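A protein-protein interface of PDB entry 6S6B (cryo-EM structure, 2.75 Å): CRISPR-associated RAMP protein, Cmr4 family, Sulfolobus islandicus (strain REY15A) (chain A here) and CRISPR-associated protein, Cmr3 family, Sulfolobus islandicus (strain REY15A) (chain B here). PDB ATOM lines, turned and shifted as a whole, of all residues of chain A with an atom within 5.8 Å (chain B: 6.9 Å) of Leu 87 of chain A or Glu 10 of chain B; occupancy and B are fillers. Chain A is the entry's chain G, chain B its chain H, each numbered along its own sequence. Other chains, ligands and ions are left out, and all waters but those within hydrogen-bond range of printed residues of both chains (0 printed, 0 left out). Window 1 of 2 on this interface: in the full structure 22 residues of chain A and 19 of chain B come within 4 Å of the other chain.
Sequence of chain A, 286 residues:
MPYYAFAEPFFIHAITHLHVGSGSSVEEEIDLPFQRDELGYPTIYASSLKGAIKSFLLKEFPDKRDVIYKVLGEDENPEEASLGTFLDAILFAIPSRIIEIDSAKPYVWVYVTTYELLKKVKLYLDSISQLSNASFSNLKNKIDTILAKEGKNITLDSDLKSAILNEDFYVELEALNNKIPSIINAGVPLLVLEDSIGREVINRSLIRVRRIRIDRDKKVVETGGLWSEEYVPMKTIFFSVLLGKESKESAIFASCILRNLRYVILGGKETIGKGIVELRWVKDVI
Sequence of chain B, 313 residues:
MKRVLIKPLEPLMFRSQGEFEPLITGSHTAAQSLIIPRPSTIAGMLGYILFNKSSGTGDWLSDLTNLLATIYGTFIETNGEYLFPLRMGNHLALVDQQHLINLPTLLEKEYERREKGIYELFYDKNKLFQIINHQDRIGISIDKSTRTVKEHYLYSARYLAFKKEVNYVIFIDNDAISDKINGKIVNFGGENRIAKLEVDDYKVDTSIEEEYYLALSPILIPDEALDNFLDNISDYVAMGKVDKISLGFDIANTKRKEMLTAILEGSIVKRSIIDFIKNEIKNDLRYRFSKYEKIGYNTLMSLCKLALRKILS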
ATOM      1  N   ILE A  44      -4.850 -25.716  17.830  1.00  0.00           N
ATOM      2  CA  ILE A  44      -4.368 -24.523  17.155  1.00  0.00           C
ATOM      3  C   ILE A  44      -3.121 -24.929  16.396  1.00  0.00           C
ATOM      4  O   ILE A  44      -2.157 -25.417  16.995  1.00  0.00           O
ATOM      5  CB  ILE A  44      -4.078 -23.388  18.144  1.00  0.00           C
ATOM      6  CG1 ILE A  44      -5.291 -23.151  19.036  1.00  0.00           C
ATOM      7  CG2 ILE A  44      -3.705 -22.129  17.404  1.00  0.00           C
ATOM      8  CD1 ILE A  44      -5.017 -22.239  20.188  1.00  0.00           C
ATOM      9  N   TYR A  45      -3.147 -24.761  15.080  1.00  0.00           N
ATOM     10  CA  TYR A  45      -1.992 -25.108  14.272  1.00  0.00           C
ATOM     11  C   TYR A  45      -0.807 -24.234  14.648  1.00  0.00           C
ATOM     12  O   TYR A  45      -0.963 -23.128  15.166  1.00  0.00           O
ATOM     13  CB  TYR A  45      -2.314 -24.950  12.794  1.00  0.00           C
ATOM     14  CG  TYR A  45      -3.326 -25.942  12.295  1.00  0.00           C
ATOM     15  CD1 TYR A  45      -3.612 -27.085  13.014  1.00  0.00           C
ATOM     16  CD2 TYR A  45      -3.993 -25.737  11.103  1.00  0.00           C
ATOM     17  CE1 TYR A  45      -4.532 -27.992  12.564  1.00  0.00           C
ATOM     18  CE2 TYR A  45      -4.913 -26.639  10.647  1.00  0.00           C
ATOM     19  CZ  TYR A  45      -5.179 -27.764  11.382  1.00  0.00           C
ATOM     20  OH  TYR A  45      -6.100 -28.671  10.927  1.00  0.00           O
ATOM     21  N   ALA A  46       0.393 -24.745  14.393  1.00  0.00           N
ATOM     22  CA  ALA A  46       1.588 -23.990  14.738  1.00  0.00           C
ATOM     23  C   ALA A  46       1.746 -22.769  13.852  1.00  0.00           C
ATOM     24  O   ALA A  46       2.349 -21.778  14.270  1.00  0.00           O
ATOM     25  CB  ALA A  46       2.817 -24.884  14.638  1.00  0.00           C
ATOM     26  N   LEU A  49      -0.761 -20.215  15.373  1.00  0.00           N
ATOM     27  CA  LEU A  49      -0.348 -19.780  16.699  1.00  0.00           C
ATOM     28  C   LEU A  49       0.891 -18.904  16.636  1.00  0.00           C
ATOM     29  O   LEU A  49       1.019 -17.956  17.415  1.00  0.00           O
ATOM     30  CB  LEU A  49      -0.105 -20.993  17.589  1.00  0.00           C
ATOM     31  CG  LEU A  49       0.592 -20.742  18.921  1.00  0.00           C
ATOM     32  CD1 LEU A  49      -0.290 -19.928  19.836  1.00  0.00           C
ATOM     33  CD2 LEU A  49       0.946 -22.059  19.560  1.00  0.00           C
ATOM     34  N   THR A  85      10.417 -22.227  17.415  1.00  0.00           N
ATOM     35  CA  THR A  85       9.372 -23.059  16.845  1.00  0.00           C
ATOM     36  C   THR A  85       8.260 -23.241  17.859  1.00  0.00           C
ATOM     37  O   THR A  85       8.517 -23.497  19.037  1.00  0.00           O
ATOM     38  CB  THR A  85       9.907 -24.427  16.429  1.00  0.00           C
ATOM     39  OG1 THR A  85      11.152 -24.265  15.743  1.00  0.00           O
ATOM     40  CG2 THR A  85       8.927 -25.126  15.517  1.00  0.00           C
ATOM     41  N   PHE A  86       7.026 -23.100  17.394  1.00  0.00           N
ATOM     42  CA  PHE A  86       5.852 -23.469  18.164  1.00  0.00           C
ATOM     43  C   PHE A  86       5.394 -24.857  17.746  1.00  0.00           C
ATOM     44  O   PHE A  86       5.427 -25.202  16.563  1.00  0.00           O
ATOM     45  CB  PHE A  86       4.714 -22.474  17.951  1.00  0.00           C
ATOM     46  CG  PHE A  86       4.921 -21.158  18.629  1.00  0.00           C
ATOM     47  CD1 PHE A  86       4.669 -21.015  19.975  1.00  0.00           C
ATOM     48  CD2 PHE A  86       5.346 -20.060  17.915  1.00  0.00           C
ATOM     49  CE1 PHE A  86       4.851 -19.806  20.597  1.00  0.00           C
ATOM     50  CE2 PHE A  86       5.528 -18.850  18.535  1.00  0.00           C
ATOM     51  CZ  PHE A  86       5.280 -18.723  19.877  1.00  0.00           C
ATOM     52  N   LEU A  87       4.977 -25.651  18.717  1.00  0.00           N
ATOM     53  CA  LEU A  87       4.278 -26.887  18.424  1.00  0.00           C
ATOM     54  C   LEU A  87       2.784 -26.615  18.392  1.00  0.00           C
ATOM     55  O   LEU A  87       2.299 -25.671  19.018  1.00  0.00           O
ATOM     56  CB  LEU A  87       4.599 -27.956  19.464  1.00  0.00           C
ATOM     57  CG  LEU A  87       6.071 -28.349  19.566  1.00  0.00           C
ATOM     58  CD1 LEU A  87       6.325 -29.126  20.828  1.00  0.00           C
ATOM     59  CD2 LEU A  87       6.462 -29.165  18.363  1.00  0.00           C
ATOM     60  N   ASP A  88       2.059 -27.435  17.633  1.00  0.00           N
ATOM     61  CA  ASP A  88       0.608 -27.319  17.594  1.00  0.00           C
ATOM     62  C   ASP A  88       0.051 -27.294  19.007  1.00  0.00           C
ATOM     63  O   ASP A  88       0.471 -28.068  19.867  1.00  0.00           O
ATOM     64  CB  ASP A  88       0.000 -28.485  16.822  1.00  0.00           C
ATOM     65  CG  ASP A  88       0.345 -28.456  15.365  1.00  0.00           C
ATOM     66  OD1 ASP A  88       0.947 -27.463  14.923  1.00  0.00           O
ATOM     67  OD2 ASP A  88       0.017 -29.428  14.658  1.00  0.00           O
ATOM     68  N   ALA A  89      -0.883 -26.385  19.252  1.00  0.00           N
ATOM     69  CA  ALA A  89      -1.518 -26.328  20.556  1.00  0.00           C
ATOM     70  C   ALA A  89      -2.467 -27.504  20.686  1.00  0.00           C
ATOM     71  O   ALA A  89      -3.262 -27.773  19.786  1.00  0.00           O
ATOM     72  CB  ALA A  89      -2.259 -25.012  20.745  1.00  0.00           C
ATOM     73  N   LEU A 123       3.485 -36.833  25.644  1.00  0.00           N
ATOM     74  CA  LEU A 123       4.432 -36.911  24.538  1.00  0.00           C
ATOM     75  C   LEU A 123       5.225 -35.618  24.402  1.00  0.00           C
ATOM     76  O   LEU A 123       6.448 -35.640  24.229  1.00  0.00           O
ATOM     77  CB  LEU A 123       3.685 -37.225  23.246  1.00  0.00           C
ATOM     78  CG  LEU A 123       4.516 -37.156  21.971  1.00  0.00           C
ATOM     79  CD1 LEU A 123       5.663 -38.130  22.058  1.00  0.00           C
ATOM     80  CD2 LEU A 123       3.657 -37.445  20.755  1.00  0.00           C
ATOM     81  N   TYR A 124       4.540 -34.476  24.471  1.00  0.00           N
ATOM     82  CA  TYR A 124       5.237 -33.197  24.455  1.00  0.00           C
ATOM     83  C   TYR A 124       6.134 -33.039  25.669  1.00  0.00           C
ATOM     84  O   TYR A 124       7.203 -32.431  25.575  1.00  0.00           O
ATOM     85  CB  TYR A 124       4.235 -32.045  24.418  1.00  0.00           C
ATOM     86  CG  TYR A 124       3.673 -31.715  23.058  1.00  0.00           C
ATOM     87  CD1 TYR A 124       3.755 -32.612  22.011  1.00  0.00           C
ATOM     88  CD2 TYR A 124       3.049 -30.500  22.831  1.00  0.00           C
ATOM     89  CE1 TYR A 124       3.235 -32.307  20.777  1.00  0.00           C
ATOM     90  CE2 TYR A 124       2.528 -30.186  21.602  1.00  0.00           C
ATOM     91  CZ  TYR A 124       2.624 -31.092  20.578  1.00  0.00           C
ATOM     92  OH  TYR A 124       2.102 -30.780  19.349  1.00  0.00           O
ATOM     93  N   ILE A 128      10.831 -32.875  25.710  1.00  0.00           N
ATOM     94  CA  ILE A 128      11.665 -31.727  26.047  1.00  0.00           C
ATOM     95  C   ILE A 128      12.306 -31.846  27.415  1.00  0.00           C
ATOM     96  O   ILE A 128      13.066 -30.946  27.802  1.00  0.00           O
ATOM     97  CB  ILE A 128      10.875 -30.409  25.948  1.00  0.00           C
ATOM     98  CG1 ILE A 128       9.853 -30.329  27.070  1.00  0.00           C
ATOM     99  CG2 ILE A 128      10.181 -30.317  24.607  1.00  0.00           C
ATOM    100  CD1 ILE A 128       8.924 -29.151  26.963  1.00  0.00           C
ATOM    101  N   PHE A 239      -2.443 -26.553  25.383  1.00  0.00           N
ATOM    102  CA  PHE A 239      -1.069 -26.663  25.836  1.00  0.00           C
ATOM    103  C   PHE A 239      -0.159 -26.755  24.624  1.00  0.00           C
ATOM    104  O   PHE A 239      -0.411 -27.551  23.716  1.00  0.00           O
ATOM    105  CB  PHE A 239      -0.898 -27.878  26.744  1.00  0.00           C
ATOM    106  CG  PHE A 239       0.524 -28.258  26.987  1.00  0.00           C
ATOM    107  CD1 PHE A 239       1.251 -27.650  27.987  1.00  0.00           C
ATOM    108  CD2 PHE A 239       1.132 -29.236  26.229  1.00  0.00           C
ATOM    109  CE1 PHE A 239       2.555 -28.002  28.213  1.00  0.00           C
ATOM    110  CE2 PHE A 239       2.436 -29.586  26.454  1.00  0.00           C
ATOM    111  CZ  PHE A 239       3.146 -28.970  27.446  1.00  0.00           C
ATOM    112  N   SER A 240       0.888 -25.939  24.605  1.00  0.00           N
ATOM    113  CA  SER A 240       1.853 -25.954  23.522  1.00  0.00           C
ATOM    114  C   SER A 240       3.233 -25.674  24.087  1.00  0.00           C
ATOM    115  O   SER A 240       3.395 -25.357  25.264  1.00  0.00           O
ATOM    116  CB  SER A 240       1.504 -24.935  22.439  1.00  0.00           C
ATOM    117  OG  SER A 240       2.348 -25.092  21.317  1.00  0.00           O
ATOM    118  N   VAL A 241       4.238 -25.796  23.229  1.00  0.00           N
ATOM    119  CA  VAL A 241       5.627 -25.587  23.608  1.00  0.00           C
ATOM    120  C   VAL A 241       6.267 -24.652  22.598  1.00  0.00           C
ATOM    121  O   VAL A 241       5.956 -24.706  21.405  1.00  0.00           O
ATOM    122  CB  VAL A 241       6.406 -26.915  23.681  1.00  0.00           C
ATOM    123  CG1 VAL A 241       7.779 -26.695  24.278  1.00  0.00           C
ATOM    124  CG2 VAL A 241       5.639 -27.947  24.481  1.00  0.00           C
ATOM    125  N   LEU A 242       7.158 -23.794  23.074  1.00  0.00           N
ATOM    126  CA  LEU A 242       7.961 -22.934  22.218  1.00  0.00           C
ATOM    127  C   LEU A 242       9.406 -23.398  22.318  1.00  0.00           C
ATOM    128  O   LEU A 242      10.049 -23.227  23.357  1.00  0.00           O
ATOM    129  CB  LEU A 242       7.825 -21.470  22.618  1.00  0.00           C
ATOM    130  CG  LEU A 242       8.816 -20.533  21.932  1.00  0.00           C
ATOM    131  CD1 LEU A 242       8.483 -20.370  20.470  1.00  0.00           C
ATOM    132  CD2 LEU A 242       8.822 -19.197  22.618  1.00  0.00           C
ATOM    133  N   LEU A 243       9.911 -23.982  21.242  1.00  0.00           N
ATOM    134  CA  LEU A 243      11.272 -24.482  21.202  1.00  0.00           C
ATOM    135  C   LEU A 243      12.200 -23.427  20.627  1.00  0.00           C
ATOM    136  O   LEU A 243      11.897 -22.810  19.603  1.00  0.00           O
ATOM    137  CB  LEU A 243      11.347 -25.750  20.360  1.00  0.00           C
ATOM    138  CG  LEU A 243      10.467 -26.900  20.812  1.00  0.00           C
ATOM    139  CD1 LEU A 243      10.106 -27.749  19.628  1.00  0.00           C
ATOM    140  CD2 LEU A 243      11.212 -27.710  21.833  1.00  0.00           C
ATOM    141  N   LYS B   7      10.462 -40.211  16.265  1.00  0.00           N
ATOM    142  CA  LYS B   7       9.100 -40.090  16.751  1.00  0.00           C
ATOM    143  C   LYS B   7       8.559 -38.714  16.413  1.00  0.00           C
ATOM    144  O   LYS B   7       8.978 -37.728  17.032  1.00  0.00           O
ATOM    145  CB  LYS B   7       9.051 -40.324  18.255  1.00  0.00           C
ATOM    146  CG  LYS B   7       7.677 -40.646  18.779  1.00  0.00           C
ATOM    147  CD  LYS B   7       7.646 -40.541  20.286  1.00  0.00           C
ATOM    148  CE  LYS B   7       6.650 -41.517  20.879  1.00  0.00           C
ATOM    149  NZ  LYS B   7       5.396 -41.558  20.084  1.00  0.00           N
ATOM    150  N   PRO B   8       7.649 -38.589  15.452  1.00  0.00           N
ATOM    151  CA  PRO B   8       7.056 -37.279  15.164  1.00  0.00           C
ATOM    152  C   PRO B   8       6.127 -36.846  16.285  1.00  0.00           C
ATOM    153  O   PRO B   8       5.225 -37.585  16.681  1.00  0.00           O
ATOM    154  CB  PRO B   8       6.291 -37.520  13.862  1.00  0.00           C
ATOM    155  CG  PRO B   8       6.024 -38.974  13.850  1.00  0.00           C
ATOM    156  CD  PRO B   8       7.189 -39.620  14.511  1.00  0.00           C
ATOM    157  N   LEU B   9       6.354 -35.638  16.797  1.00  0.00           N
ATOM    158  CA  LEU B   9       5.520 -35.095  17.858  1.00  0.00           C
ATOM    159  C   LEU B   9       4.254 -34.442  17.332  1.00  0.00           C
ATOM    160  O   LEU B   9       3.397 -34.053  18.130  1.00  0.00           O
ATOM    161  CB  LEU B   9       6.300 -34.070  18.675  1.00  0.00           C
ATOM    162  CG  LEU B   9       7.735 -34.435  19.021  1.00  0.00           C
ATOM    163  CD1 LEU B   9       8.310 -33.399  19.954  1.00  0.00           C
ATOM    164  CD2 LEU B   9       7.789 -35.810  19.649  1.00  0.00           C
ATOM    165  N   GLU B  10       4.116 -34.324  16.021  1.00  0.00           N
ATOM    166  CA  GLU B  10       3.041 -33.570  15.399  1.00  0.00           C
ATOM    167  C   GLU B  10       3.075 -33.860  13.908  1.00  0.00           C
ATOM    168  O   GLU B  10       4.096 -34.321  13.399  1.00  0.00           O
ATOM    169  CB  GLU B  10       3.194 -32.067  15.661  1.00  0.00           C
ATOM    170  CG  GLU B  10       4.438 -31.465  15.050  1.00  0.00           C
ATOM    171  CD  GLU B  10       4.619 -30.016  15.434  1.00  0.00           C
ATOM    172  OE1 GLU B  10       3.841 -29.525  16.273  1.00  0.00           O
ATOM    173  OE2 GLU B  10       5.541 -29.368  14.905  1.00  0.00           O
ATOM    174  N   PRO B  11       1.972 -33.624  13.201  1.00  0.00           N
ATOM    175  CA  PRO B  11       1.955 -33.882  11.759  1.00  0.00           C
ATOM    176  C   PRO B  11       3.148 -33.252  11.058  1.00  0.00           C
ATOM    177  O   PRO B  11       3.551 -32.130  11.361  1.00  0.00           O
ATOM    178  CB  PRO B  11       0.639 -33.249  11.310  1.00  0.00           C
ATOM    179  CG  PRO B  11      -0.225 -33.363  12.483  1.00  0.00           C
ATOM    180  CD  PRO B  11       0.644 -33.231  13.694  1.00  0.00           C
ATOM    181  N   LEU B  12       3.723 -34.000  10.130  1.00  0.00           N
ATOM    182  CA  LEU B  12       4.886 -33.580   9.370  1.00  0.00           C
ATOM    183  C   LEU B  12       4.494 -33.373   7.918  1.00  0.00           C
ATOM    184  O   LEU B  12       3.397 -33.725   7.489  1.00  0.00           O
ATOM    185  CB  LEU B  12       6.000 -34.624   9.460  1.00  0.00           C
ATOM    186  CG  LEU B  12       6.343 -35.180  10.836  1.00  0.00           C
ATOM    187  CD1 LEU B  12       7.186 -36.414  10.670  1.00  0.00           C
ATOM    188  CD2 LEU B  12       7.070 -34.149  11.667  1.00  0.00           C
ATOM    189  N   MET B  13       5.413 -32.795   7.158  1.00  0.00           N
ATOM    190  CA  MET B  13       5.243 -32.688   5.718  1.00  0.00           C
ATOM    191  C   MET B  13       6.600 -32.855   5.060  1.00  0.00           C
ATOM    192  O   MET B  13       7.514 -32.076   5.322  1.00  0.00           O
ATOM    193  CB  MET B  13       4.620 -31.351   5.319  1.00  0.00           C
ATOM    194  CG  MET B  13       4.083 -31.356   3.905  1.00  0.00           C
ATOM    195  SD  MET B  13       3.629 -29.742   3.302  1.00  0.00           S
ATOM    196  CE  MET B  13       5.252 -29.106   2.926  1.00  0.00           C
ATOM    197  N   ARG B 137      -4.008 -29.020   5.755  1.00  0.00           N
ATOM    198  CA  ARG B 137      -3.953 -27.686   6.333  1.00  0.00           C
ATOM    199  C   ARG B 137      -3.923 -26.639   5.235  1.00  0.00           C
ATOM    200  O   ARG B 137      -3.299 -26.828   4.193  1.00  0.00           O
ATOM    201  CB  ARG B 137      -2.724 -27.530   7.216  1.00  0.00           C
ATOM    202  CG  ARG B 137      -2.678 -28.497   8.356  1.00  0.00           C
ATOM    203  CD  ARG B 137      -1.510 -28.222   9.253  1.00  0.00           C
ATOM    204  NE  ARG B 137      -1.592 -29.015  10.469  1.00  0.00           N
ATOM    205  CZ  ARG B 137      -0.929 -28.733  11.579  1.00  0.00           C
ATOM    206  NH1 ARG B 137      -0.135 -27.679  11.624  1.00  0.00           N
ATOM    207  NH2 ARG B 137      -1.063 -29.502  12.643  1.00  0.00           N
ATOM    208  N   TYR B 159      -0.582 -32.188   5.181  1.00  0.00           N
ATOM    209  CA  TYR B 159       0.390 -32.690   6.137  1.00  0.00           C
ATOM    210  C   TYR B 159       0.235 -34.199   6.268  1.00  0.00           C
ATOM    211  O   TYR B 159      -0.556 -34.840   5.575  1.00  0.00           O
ATOM    212  CB  TYR B 159       0.221 -31.999   7.481  1.00  0.00           C
ATOM    213  CG  TYR B 159       0.911 -30.669   7.582  1.00  0.00           C
ATOM    214  CD1 TYR B 159       0.626 -29.654   6.694  1.00  0.00           C
ATOM    215  CD2 TYR B 159       1.844 -30.429   8.568  1.00  0.00           C
ATOM    216  CE1 TYR B 159       1.248 -28.443   6.785  1.00  0.00           C
ATOM    217  CE2 TYR B 159       2.470 -29.220   8.667  1.00  0.00           C
ATOM    218  CZ  TYR B 159       2.168 -28.231   7.773  1.00  0.00           C
ATOM    219  OH  TYR B 159       2.791 -27.015   7.866  1.00  0.00           O
ATOM    220  N   LEU B 160       0.995 -34.780   7.186  1.00  0.00           N
ATOM    221  CA  LEU B 160       0.980 -36.210   7.451  1.00  0.00           C
ATOM    222  C   LEU B 160       0.523 -36.396   8.890  1.00  0.00           C
ATOM    223  O   LEU B 160       1.334 -36.378   9.814  1.00  0.00           O
ATOM    224  CB  LEU B 160       2.342 -36.803   7.225  1.00  0.00           C
ATOM    225  CG  LEU B 160       2.390 -38.196   6.623  1.00  0.00           C
ATOM    226  CD1 LEU B 160       1.557 -38.226   5.368  1.00  0.00           C
ATOM    227  CD2 LEU B 160       3.821 -38.543   6.325  1.00  0.00           C
ATOM    228  N   ALA B 161      -0.777 -36.566   9.080  1.00  0.00           N
ATOM    229  CA  ALA B 161      -1.331 -36.781  10.404  1.00  0.00           C
ATOM    230  C   ALA B 161      -1.242 -38.256  10.763  1.00  0.00           C
ATOM    231  O   ALA B 161      -1.501 -39.124   9.928  1.00  0.00           O
ATOM    232  CB  ALA B 161      -2.783 -36.311  10.465  1.00  0.00           C
ATOM    233  N   PHE B 162      -0.876 -38.532  12.010  1.00  0.00           N
ATOM    234  CA  PHE B 162      -0.663 -39.893  12.487  1.00  0.00           C
ATOM    235  C   PHE B 162      -1.764 -40.247  13.474  1.00  0.00           C
ATOM    236  O   PHE B 162      -1.817 -39.696  14.576  1.00  0.00           O
ATOM    237  CB  PHE B 162       0.711 -40.028  13.127  1.00  0.00           C
ATOM    238  CG  PHE B 162       1.827 -39.587  12.240  1.00  0.00           C
ATOM    239  CD1 PHE B 162       2.240 -40.379  11.187  1.00  0.00           C
ATOM    240  CD2 PHE B 162       2.456 -38.377  12.449  1.00  0.00           C
ATOM    241  CE1 PHE B 162       3.262 -39.976  10.368  1.00  0.00           C
ATOM    242  CE2 PHE B 162       3.478 -37.969  11.631  1.00  0.00           C
ATOM    243  CZ  PHE B 162       3.882 -38.769  10.589  1.00  0.00           C
ATOM    244  N   ILE B 185      15.775 -33.450  20.325  1.00  0.00           N
ATOM    245  CA  ILE B 185      14.670 -32.836  19.603  1.00  0.00           C
ATOM    246  C   ILE B 185      15.209 -32.332  18.275  1.00  0.00           C
ATOM    247  O   ILE B 185      16.112 -31.491  18.241  1.00  0.00           O
ATOM    248  CB  ILE B 185      14.043 -31.696  20.414  1.00  0.00           C
ATOM    249  CG1 ILE B 185      13.183 -32.258  21.536  1.00  0.00           C
ATOM    250  CG2 ILE B 185      13.213 -30.808  19.522  1.00  0.00           C
ATOM    251  CD1 ILE B 185      11.984 -33.001  21.047  1.00  0.00           C
ATOM    252  N   GLU B 191       7.733 -28.247   7.209  1.00  0.00           N
ATOM    253  CA  GLU B 191       7.354 -26.860   7.474  1.00  0.00           C
ATOM    254  C   GLU B 191       7.687 -26.462   8.905  1.00  0.00           C
ATOM    255  O   GLU B 191       6.822 -26.036   9.664  1.00  0.00           O
ATOM    256  CB  GLU B 191       5.873 -26.658   7.188  1.00  0.00           C
ATOM    257  CG  GLU B 191       5.479 -26.876   5.744  1.00  0.00           C
ATOM    258  CD  GLU B 191       5.890 -25.728   4.837  1.00  0.00           C
ATOM    259  OE1 GLU B 191       6.702 -25.960   3.917  1.00  0.00           O
ATOM    260  OE2 GLU B 191       5.400 -24.596   5.037  1.00  0.00           O
ATOM    261  N   ASN B 192       8.954 -26.624   9.281  1.00  0.00           N
ATOM    262  CA  ASN B 192       9.440 -26.294  10.619  1.00  0.00           C
ATOM    263  C   ASN B 192       8.782 -27.166  11.685  1.00  0.00           C
ATOM    264  O   ASN B 192       8.375 -26.677  12.734  1.00  0.00           O
ATOM    265  CB  ASN B 192       9.240 -24.812  10.938  1.00  0.00           C
ATOM    266  CG  ASN B 192      10.315 -24.268  11.838  1.00  0.00           C
ATOM    267  OD1 ASN B 192      11.499 -24.505  11.620  1.00  0.00           O
ATOM    268  ND2 ASN B 192       9.912 -23.525  12.856  1.00  0.00           N
ATOM    269  N   ARG B 193       8.693 -28.464  11.421  1.00  0.00           N
ATOM    270  CA  ARG B 193       8.068 -29.403  12.335  1.00  0.00           C
ATOM    271  C   ARG B 193       9.131 -30.067  13.205  1.00  0.00           C
ATOM    272  O   ARG B 193      10.329 -29.836  13.047  1.00  0.00           O
ATOM    273  CB  ARG B 193       7.253 -30.429  11.555  1.00  0.00           C
ATOM    274  CG  ARG B 193       6.468 -29.823  10.414  1.00  0.00           C
ATOM    275  CD  ARG B 193       5.383 -28.910  10.930  1.00  0.00           C
ATOM    276  NE  ARG B 193       4.264 -29.661  11.482  1.00  0.00           N
ATOM    277  CZ  ARG B 193       3.386 -29.166  12.345  1.00  0.00           C
ATOM    278  NH1 ARG B 193       3.498 -27.916  12.759  1.00  0.00           N
ATOM    279  NH2 ARG B 193       2.402 -29.921  12.795  1.00  0.00           N
ATOM    280  N   ILE B 194       8.687 -30.900  14.140  1.00  0.00           N
ATOM    281  CA  ILE B 194       9.551 -31.401  15.203  1.00  0.00           C
ATOM    282  C   ILE B 194       9.318 -32.891  15.392  1.00  0.00           C
ATOM    283  O   ILE B 194       8.171 -33.345  15.438  1.00  0.00           O
ATOM    284  CB  ILE B 194       9.306 -30.661  16.530  1.00  0.00           C
ATOM    285  CG1 ILE B 194       9.586 -29.175  16.366  1.00  0.00           C
ATOM    286  CG2 ILE B 194      10.177 -31.224  17.621  1.00  0.00           C
ATOM    287  CD1 ILE B 194      11.026 -28.872  16.192  1.00  0.00           C
ATOM    288  N   ALA B 195      10.405 -33.647  15.515  1.00  0.00           N
ATOM    289  CA  ALA B 195      10.364 -35.048  15.894  1.00  0.00           C
ATOM    290  C   ALA B 195      11.405 -35.294  16.974  1.00  0.00           C
ATOM    291  O   ALA B 195      12.288 -34.470  17.214  1.00  0.00           O
ATOM    292  CB  ALA B 195      10.612 -35.965  14.694  1.00  0.00           C
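The side-chain hydroxyl (OG1) of Thr 85 of chain A is in hydrogen-bond range of the side-chain amide nitrogen (ND2) of Asn 192 of chain B (3.2 Å). The side-chain carboxylate of Glu 10 of chain B sits at hydrogen-bond distance from the backbone NH of Asp 88 of chain A (3.1 Å). The side-chain carboxylate (OD1) of Asp 88 of chain A is in salt-bridge range of the guanidinium group (NH1) of Arg 137 of chain B, at 3.5 Å. The side-chain carboxylate (OD2) of Asp 88 of chain A lies within salt-bridge range of the guanidinium group (NH2) of Arg 193 of chain B (3.1 Å).
The side-chain carboxylate (OD1) of Asp 88 of chain A is in hydrogen-bond range of the backbone NH (N) of Ala 46 of chain A (2.8 Å). The backbone NH (N) of Leu 243 of chain A is in hydrogen-bond range of the backbone carbonyl oxygen (O) of Thr 85 of chain A. The backbone NH (N) of Leu 87 of chain A lies within hydrogen-bond range of the backbone carbonyl oxygen (O) of Val 241 of chain A (3.0 Å). The backbone carbonyl oxygen (O) of Asp 88 of chain A lies within hydrogen-bond range of the side-chain hydroxyl (OH) of Tyr 124 of chain A (3.2 Å). N of Leu 9 of chain B lies within hydrogen-bond range of O of Ile 194 of chain B (3.2 Å). OE2 of Glu 10 of chain B is in salt-bridge range of NH1 of Arg 193 of chain B (3.3 Å).
Hydrophobic or aromatic side chains of chain A within 4 Å of the printed part of chain B: Tyr 45, Ala 46, Leu 87, Leu 123, Tyr 124 and Leu 243. Of the 18 printed residues of chain B, 8 touch a printed residue of chain A. Among the printed residues, Asp or Glu carboxylates within 4 Å of a Lys or Arg side-chain nitrogen of the other chain: Asp 88 of chain A with Arg 137 of chain B (2.3 Å) and Asp 88 of chain A with Arg 193 of chain B (3.1 Å).
Printed residues of chain B within 4 Å of Thr 85 of chain A: Asn 192. Of the printed residues of chain B, Leu 87 of chain A touches Glu 10 and Ile 194. Of chain A, only Leu 87, Asp 88 and Tyr 124 come within 4 Å of Glu 10 of chain B. Printed residues of chain A within 4 Å of Arg 137 of chain B: Tyr 45 (3.5 Å) and Asp 88 (2.3 Å). Ala 161 of chain B touches none of the printed residues of chain A. Phe 162 of chain B touches none of the printed residues of chain A. Of the printed residues of chain A, Arg 193 of chain B touches Ala 46 and Asp 88.
Tyr 45 of chain A touches Arg 137 of chain B (CD1 to CZ, 3.5 Å). Arg 193 of chain B touches Ala 46 of chain A (NH1 to CB, 3.6 Å). CD2 of Leu 87 of chain A touches OE1 of Glu 10 of chain B, 3.4 Å away. Ile 194 of chain B touches Leu 87 of chain A. OD2 of Asp 88 of chain A touches CD of Pro 11 of chain B, 3.97 Å away. Leu 123 of chain A touches Lys 7 of chain B. CD1 of Leu 123 of chain A touches CD2 of Leu 9 of chain B, 3.96 Å away. O of Leu 9 of chain B touches CE1 of Tyr 124 of chain A (3.2 Å). Tyr 124 of chain A touches Glu 10 of chain B. Leu 243 of chain A touches Ile 194 of chain B.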
